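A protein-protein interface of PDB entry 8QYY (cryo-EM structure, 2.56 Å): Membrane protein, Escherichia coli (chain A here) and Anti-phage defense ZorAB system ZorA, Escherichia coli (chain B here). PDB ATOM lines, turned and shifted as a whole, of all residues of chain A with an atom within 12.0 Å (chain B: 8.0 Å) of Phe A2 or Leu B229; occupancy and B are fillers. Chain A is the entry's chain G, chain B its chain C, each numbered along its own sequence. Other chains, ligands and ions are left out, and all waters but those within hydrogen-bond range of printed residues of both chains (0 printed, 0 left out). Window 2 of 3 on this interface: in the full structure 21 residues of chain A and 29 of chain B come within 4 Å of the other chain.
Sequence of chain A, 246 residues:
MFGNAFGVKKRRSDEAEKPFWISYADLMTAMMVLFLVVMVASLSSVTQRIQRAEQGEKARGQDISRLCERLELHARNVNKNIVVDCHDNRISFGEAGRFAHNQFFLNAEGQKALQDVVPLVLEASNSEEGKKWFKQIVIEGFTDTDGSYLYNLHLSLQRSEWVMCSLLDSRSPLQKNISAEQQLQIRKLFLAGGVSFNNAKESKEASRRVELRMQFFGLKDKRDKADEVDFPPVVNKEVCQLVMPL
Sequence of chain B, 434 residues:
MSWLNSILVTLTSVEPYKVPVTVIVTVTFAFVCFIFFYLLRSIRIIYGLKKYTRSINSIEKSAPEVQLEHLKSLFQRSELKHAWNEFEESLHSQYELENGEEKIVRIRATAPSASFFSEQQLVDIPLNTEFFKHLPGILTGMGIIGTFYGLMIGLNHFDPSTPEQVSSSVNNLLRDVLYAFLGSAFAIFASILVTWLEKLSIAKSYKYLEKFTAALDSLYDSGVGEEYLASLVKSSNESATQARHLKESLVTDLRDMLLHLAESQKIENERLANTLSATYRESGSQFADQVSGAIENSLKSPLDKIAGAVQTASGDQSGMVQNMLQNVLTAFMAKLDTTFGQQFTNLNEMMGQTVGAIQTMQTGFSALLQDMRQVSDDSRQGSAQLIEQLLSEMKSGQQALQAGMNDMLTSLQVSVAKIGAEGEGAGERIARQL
Among the printed residues, pairs that only touch across the chains: Phe A2 with Gly B225 (3.5 Å), Phe A2 with Glu B226 (3.1 Å), Phe A2 with Leu B229 (3.5 Å) and Asn A4 with Ala B111 (3.3 Å).
Of the 7 printed residues of chain A, 2 touch a printed residue of chain B.
Hydrophobic or aromatic side chains of chain A that line the printed part of chain B: Phe A2.
Among the printed residues, no Asp or Glu carboxylate lies within 4 Å of a Lys or Arg side-chain nitrogen of the other chain.
OD1 of Asn A4 sits at hydrogen-bond distance from N of Phe A6 (3.0 Å).
The side-chain amide nitrogen of Asn A4 lies close to the backbone NH of Gly A7.
Phe A2 touches three residues of chain B.
Leu B229 touches just one residue of chain A: Phe A2 (3.5 Å).
No residue of chain B comes within 4 Å of Gly A3.
Gly B225 touches just one residue of chain A: Phe A2.
Glu B226 touches just one residue of chain A: Phe A2.
No residue of chain A comes within 4 Å of Ala B230.
No residue of chain A comes within 4 Å of Ser B231.
Of the printed residues of chain B, Asn A4 touches Ala B111 (3.3 Å).
Of the printed residues of chain A, Ala B111 touches Asn A4.
Ser B236 touches none of the printed residues of chain A.
The nearest printed residue of chain B that does not touch Asn A4 is Thr B110 (4.1 Å).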
ATOM      1  N   MET A   1      13.487 -13.999   8.287  1.00  0.00           N
ATOM      2  CA  MET A   1      13.463 -15.028   9.318  1.00  0.00           C
ATOM      3  C   MET A   1      12.714 -16.270   8.854  1.00  0.00           C
ATOM      4  O   MET A   1      13.085 -17.391   9.199  1.00  0.00           O
ATOM      5  CB  MET A   1      12.835 -14.482  10.603  1.00  0.00           C
ATOM      6  CG  MET A   1      12.870 -15.452  11.773  1.00  0.00           C
ATOM      7  SD  MET A   1      14.545 -15.854  12.294  1.00  0.00           S
ATOM      8  CE  MET A   1      15.030 -14.327  13.079  1.00  0.00           C
ATOM      9  N   PHE A   2      11.664 -16.068   8.064  1.00  0.00           N
ATOM     10  CA  PHE A   2      10.846 -17.184   7.608  1.00  0.00           C
ATOM     11  C   PHE A   2      10.711 -17.180   6.093  1.00  0.00           C
ATOM     12  O   PHE A   2       9.612 -17.362   5.558  1.00  0.00           O
ATOM     13  CB  PHE A   2       9.475 -17.137   8.281  1.00  0.00           C
ATOM     14  CG  PHE A   2       9.511 -17.522   9.728  1.00  0.00           C
ATOM     15  CD1 PHE A   2       9.606 -18.846  10.101  1.00  0.00           C
ATOM     16  CD2 PHE A   2       9.493 -16.555  10.715  1.00  0.00           C
ATOM     17  CE1 PHE A   2       9.657 -19.201  11.430  1.00  0.00           C
ATOM     18  CE2 PHE A   2       9.541 -16.904  12.044  1.00  0.00           C
ATOM     19  CZ  PHE A   2       9.626 -18.230  12.402  1.00  0.00           C
ATOM     20  N   GLY A   3      11.825 -16.971   5.396  1.00  0.00           N
ATOM     21  CA  GLY A   3      11.804 -17.002   3.952  1.00  0.00           C
ATOM     22  C   GLY A   3      11.656 -18.407   3.409  1.00  0.00           C
ATOM     23  O   GLY A   3      11.923 -19.404   4.081  1.00  0.00           O
ATOM     24  N   ASN A   4      11.216 -18.483   2.158  1.00  0.00           N
ATOM     25  CA  ASN A   4      11.002 -19.756   1.481  1.00  0.00           C
ATOM     26  C   ASN A   4      12.265 -20.117   0.708  1.00  0.00           C
ATOM     27  O   ASN A   4      12.656 -19.408  -0.226  1.00  0.00           O
ATOM     28  CB  ASN A   4       9.790 -19.674   0.558  1.00  0.00           C
ATOM     29  CG  ASN A   4       9.654 -20.889  -0.333  1.00  0.00           C
ATOM     30  OD1 ASN A   4       9.886 -22.019   0.097  1.00  0.00           O
ATOM     31  ND2 ASN A   4       9.271 -20.665  -1.584  1.00  0.00           N
ATOM     32  N   ALA A   5      12.907 -21.219   1.099  1.00  0.00           N
ATOM     33  CA  ALA A   5      14.111 -21.660   0.410  1.00  0.00           C
ATOM     34  C   ALA A   5      13.809 -22.282  -0.945  1.00  0.00           C
ATOM     35  O   ALA A   5      14.712 -22.386  -1.779  1.00  0.00           O
ATOM     36  CB  ALA A   5      14.879 -22.661   1.274  1.00  0.00           C
ATOM     37  N   PHE A   6      12.565 -22.682  -1.183  1.00  0.00           N
ATOM     38  CA  PHE A   6      12.194 -23.394  -2.395  1.00  0.00           C
ATOM     39  C   PHE A   6      11.695 -22.478  -3.502  1.00  0.00           C
ATOM     40  O   PHE A   6      11.259 -22.977  -4.545  1.00  0.00           O
ATOM     41  CB  PHE A   6      11.139 -24.455  -2.074  1.00  0.00           C
ATOM     42  CG  PHE A   6      11.666 -25.588  -1.248  1.00  0.00           C
ATOM     43  CD1 PHE A   6      11.687 -25.506   0.130  1.00  0.00           C
ATOM     44  CD2 PHE A   6      12.170 -26.723  -1.852  1.00  0.00           C
ATOM     45  CE1 PHE A   6      12.184 -26.540   0.890  1.00  0.00           C
ATOM     46  CE2 PHE A   6      12.668 -27.761  -1.096  1.00  0.00           C
ATOM     47  CZ  PHE A   6      12.676 -27.668   0.275  1.00  0.00           C
ATOM     48  N   GLY A   7      11.736 -21.163  -3.305  1.00  0.00           N
ATOM     49  CA  GLY A   7      11.408 -20.244  -4.373  1.00  0.00           C
ATOM     50  C   GLY A   7      12.360 -20.391  -5.543  1.00  0.00           C
ATOM     51  O   GLY A   7      13.577 -20.258  -5.380  1.00  0.00           O
ATOM     52  N   THR B 110       3.553 -22.690   3.635  1.00  0.00           N
ATOM     53  CA  THR B 110       4.860 -22.142   3.961  1.00  0.00           C
ATOM     54  C   THR B 110       5.643 -21.718   2.728  1.00  0.00           C
ATOM     55  O   THR B 110       6.792 -21.288   2.858  1.00  0.00           O
ATOM     56  CB  THR B 110       5.674 -23.160   4.763  1.00  0.00           C
ATOM     57  OG1 THR B 110       5.826 -24.361   3.997  1.00  0.00           O
ATOM     58  CG2 THR B 110       4.966 -23.487   6.063  1.00  0.00           C
ATOM     59  N   ALA B 111       5.050 -21.823   1.542  1.00  0.00           N
ATOM     60  CA  ALA B 111       5.705 -21.443   0.300  1.00  0.00           C
ATOM     61  C   ALA B 111       4.632 -21.136  -0.727  1.00  0.00           C
ATOM     62  O   ALA B 111       3.523 -21.670  -0.630  1.00  0.00           O
ATOM     63  CB  ALA B 111       6.625 -22.560  -0.208  1.00  0.00           C
ATOM     64  N   GLY B 223       2.155 -17.434   7.048  1.00  0.00           N
ATOM     65  CA  GLY B 223       2.513 -16.805   8.301  1.00  0.00           C
ATOM     66  C   GLY B 223       2.437 -17.694   9.515  1.00  0.00           C
ATOM     67  O   GLY B 223       2.277 -17.187  10.628  1.00  0.00           O
ATOM     68  N   VAL B 224       2.542 -19.013   9.341  1.00  0.00           N
ATOM     69  CA  VAL B 224       2.420 -19.918  10.478  1.00  0.00           C
ATOM     70  C   VAL B 224       3.632 -19.813  11.401  1.00  0.00           C
ATOM     71  O   VAL B 224       3.497 -19.940  12.623  1.00  0.00           O
ATOM     72  CB  VAL B 224       2.185 -21.359   9.987  1.00  0.00           C
ATOM     73  CG1 VAL B 224       3.388 -21.890   9.224  1.00  0.00           C
ATOM     74  CG2 VAL B 224       1.827 -22.266  11.144  1.00  0.00           C
ATOM     75  N   GLY B 225       4.825 -19.578  10.850  1.00  0.00           N
ATOM     76  CA  GLY B 225       6.011 -19.499  11.686  1.00  0.00           C
ATOM     77  C   GLY B 225       6.005 -18.299  12.615  1.00  0.00           C
ATOM     78  O   GLY B 225       6.397 -18.402  13.782  1.00  0.00           O
ATOM     79  N   GLU B 226       5.570 -17.146  12.109  1.00  0.00           N
ATOM     80  CA  GLU B 226       5.457 -15.963  12.956  1.00  0.00           C
ATOM     81  C   GLU B 226       4.427 -16.176  14.055  1.00  0.00           C
ATOM     82  O   GLU B 226       4.624 -15.738  15.193  1.00  0.00           O
ATOM     83  CB  GLU B 226       5.098 -14.746  12.108  1.00  0.00           C
ATOM     84  CG  GLU B 226       6.282 -14.114  11.401  1.00  0.00           C
ATOM     85  CD  GLU B 226       6.596 -14.782  10.075  1.00  0.00           C
ATOM     86  OE1 GLU B 226       5.826 -15.669   9.653  1.00  0.00           O
ATOM     87  OE2 GLU B 226       7.614 -14.414   9.452  1.00  0.00           O
ATOM     88  N   GLU B 227       3.317 -16.844  13.734  1.00  0.00           N
ATOM     89  CA  GLU B 227       2.321 -17.160  14.751  1.00  0.00           C
ATOM     90  C   GLU B 227       2.892 -18.090  15.812  1.00  0.00           C
ATOM     91  O   GLU B 227       2.619 -17.922  17.005  1.00  0.00           O
ATOM     92  CB  GLU B 227       1.089 -17.781  14.101  1.00  0.00           C
ATOM     93  CG  GLU B 227       0.349 -16.845  13.173  1.00  0.00           C
ATOM     94  CD  GLU B 227      -0.851 -17.497  12.530  1.00  0.00           C
ATOM     95  OE1 GLU B 227      -1.132 -18.670  12.853  1.00  0.00           O
ATOM     96  OE2 GLU B 227      -1.516 -16.839  11.703  1.00  0.00           O
ATOM     97  N   TYR B 228       3.685 -19.079  15.395  1.00  0.00           N
ATOM     98  CA  TYR B 228       4.317 -19.972  16.358  1.00  0.00           C
ATOM     99  C   TYR B 228       5.277 -19.217  17.267  1.00  0.00           C
ATOM    100  O   TYR B 228       5.309 -19.452  18.480  1.00  0.00           O
ATOM    101  CB  TYR B 228       5.052 -21.094  15.627  1.00  0.00           C
ATOM    102  CG  TYR B 228       4.154 -22.187  15.108  1.00  0.00           C
ATOM    103  CD1 TYR B 228       2.937 -22.455  15.710  1.00  0.00           C
ATOM    104  CD2 TYR B 228       4.530 -22.958  14.020  1.00  0.00           C
ATOM    105  CE1 TYR B 228       2.119 -23.453  15.240  1.00  0.00           C
ATOM    106  CE2 TYR B 228       3.722 -23.960  13.545  1.00  0.00           C
ATOM    107  CZ  TYR B 228       2.515 -24.203  14.157  1.00  0.00           C
ATOM    108  OH  TYR B 228       1.699 -25.202  13.688  1.00  0.00           O
ATOM    109  N   LEU B 229       6.073 -18.310  16.700  1.00  0.00           N
ATOM    110  CA  LEU B 229       6.997 -17.532  17.520  1.00  0.00           C
ATOM    111  C   LEU B 229       6.251 -16.617  18.486  1.00  0.00           C
ATOM    112  O   LEU B 229       6.671 -16.447  19.638  1.00  0.00           O
ATOM    113  CB  LEU B 229       7.942 -16.724  16.635  1.00  0.00           C
ATOM    114  CG  LEU B 229       9.138 -17.478  16.055  1.00  0.00           C
ATOM    115  CD1 LEU B 229      10.141 -16.499  15.488  1.00  0.00           C
ATOM    116  CD2 LEU B 229       9.784 -18.355  17.105  1.00  0.00           C
ATOM    117  N   ALA B 230       5.150 -16.014  18.037  1.00  0.00           N
ATOM    118  CA  ALA B 230       4.343 -15.187  18.928  1.00  0.00           C
ATOM    119  C   ALA B 230       3.756 -16.013  20.063  1.00  0.00           C
ATOM    120  O   ALA B 230       3.732 -15.571  21.219  1.00  0.00           O
ATOM    121  CB  ALA B 230       3.233 -14.497  18.137  1.00  0.00           C
ATOM    122  N   SER B 231       3.283 -17.221  19.749  1.00  0.00           N
ATOM    123  CA  SER B 231       2.793 -18.121  20.784  1.00  0.00           C
ATOM    124  C   SER B 231       3.894 -18.470  21.774  1.00  0.00           C
ATOM    125  O   SER B 231       3.654 -18.538  22.981  1.00  0.00           O
ATOM    126  CB  SER B 231       2.226 -19.388  20.152  1.00  0.00           C
ATOM    127  OG  SER B 231       0.919 -19.169  19.656  1.00  0.00           O
ATOM    128  N   LEU B 232       5.110 -18.703  21.278  1.00  0.00           N
ATOM    129  CA  LEU B 232       6.218 -19.038  22.166  1.00  0.00           C
ATOM    130  C   LEU B 232       6.563 -17.878  23.092  1.00  0.00           C
ATOM    131  O   LEU B 232       6.826 -18.085  24.281  1.00  0.00           O
ATOM    132  CB  LEU B 232       7.438 -19.450  21.344  1.00  0.00           C
ATOM    133  CG  LEU B 232       7.358 -20.832  20.701  1.00  0.00           C
ATOM    134  CD1 LEU B 232       8.517 -21.039  19.756  1.00  0.00           C
ATOM    135  CD2 LEU B 232       7.341 -21.902  21.766  1.00  0.00           C
ATOM    136  N   VAL B 233       6.568 -16.653  22.567  1.00  0.00           N
ATOM    137  CA  VAL B 233       6.877 -15.488  23.396  1.00  0.00           C
ATOM    138  C   VAL B 233       5.807 -15.297  24.467  1.00  0.00           C
ATOM    139  O   VAL B 233       6.110 -15.067  25.651  1.00  0.00           O
ATOM    140  CB  VAL B 233       7.030 -14.236  22.516  1.00  0.00           C
ATOM    141  CG1 VAL B 233       7.094 -12.992  23.371  1.00  0.00           C
ATOM    142  CG2 VAL B 233       8.268 -14.352  21.655  1.00  0.00           C
ATOM    143  N   LYS B 234       4.537 -15.400  24.069  1.00  0.00           N
ATOM    144  CA  LYS B 234       3.459 -15.265  25.038  1.00  0.00           C
ATOM    145  C   LYS B 234       3.529 -16.365  26.089  1.00  0.00           C
ATOM    146  O   LYS B 234       3.297 -16.115  27.276  1.00  0.00           O
ATOM    147  CB  LYS B 234       2.106 -15.282  24.331  1.00  0.00           C
ATOM    148  CG  LYS B 234       0.927 -15.103  25.271  1.00  0.00           C
ATOM    149  CD  LYS B 234      -0.376 -14.982  24.515  1.00  0.00           C
ATOM    150  CE  LYS B 234      -0.775 -16.314  23.918  1.00  0.00           C
ATOM    151  NZ  LYS B 234      -1.143 -17.291  24.978  1.00  0.00           N
ATOM    152  N   SER B 235       3.860 -17.589  25.670  1.00  0.00           N
ATOM    153  CA  SER B 235       3.986 -18.694  26.613  1.00  0.00           C
ATOM    154  C   SER B 235       5.128 -18.464  27.589  1.00  0.00           C
ATOM    155  O   SER B 235       5.014 -18.806  28.764  1.00  0.00           O
ATOM    156  CB  SER B 235       4.184 -20.006  25.860  1.00  0.00           C
ATOM    157  OG  SER B 235       2.970 -20.454  25.293  1.00  0.00           O
ATOM    158  N   SER B 236       6.243 -17.902  27.121  1.00  0.00           N
ATOM    159  CA  SER B 236       7.357 -17.618  28.021  1.00  0.00           C
ATOM    160  C   SER B 236       6.961 -16.598  29.083  1.00  0.00           C
ATOM    161  O   SER B 236       7.230 -16.783  30.279  1.00  0.00           O
ATOM    162  CB  SER B 236       8.559 -17.121  27.223  1.00  0.00           C
ATOM    163  OG  SER B 236       9.081 -18.151  26.409  1.00  0.00           O
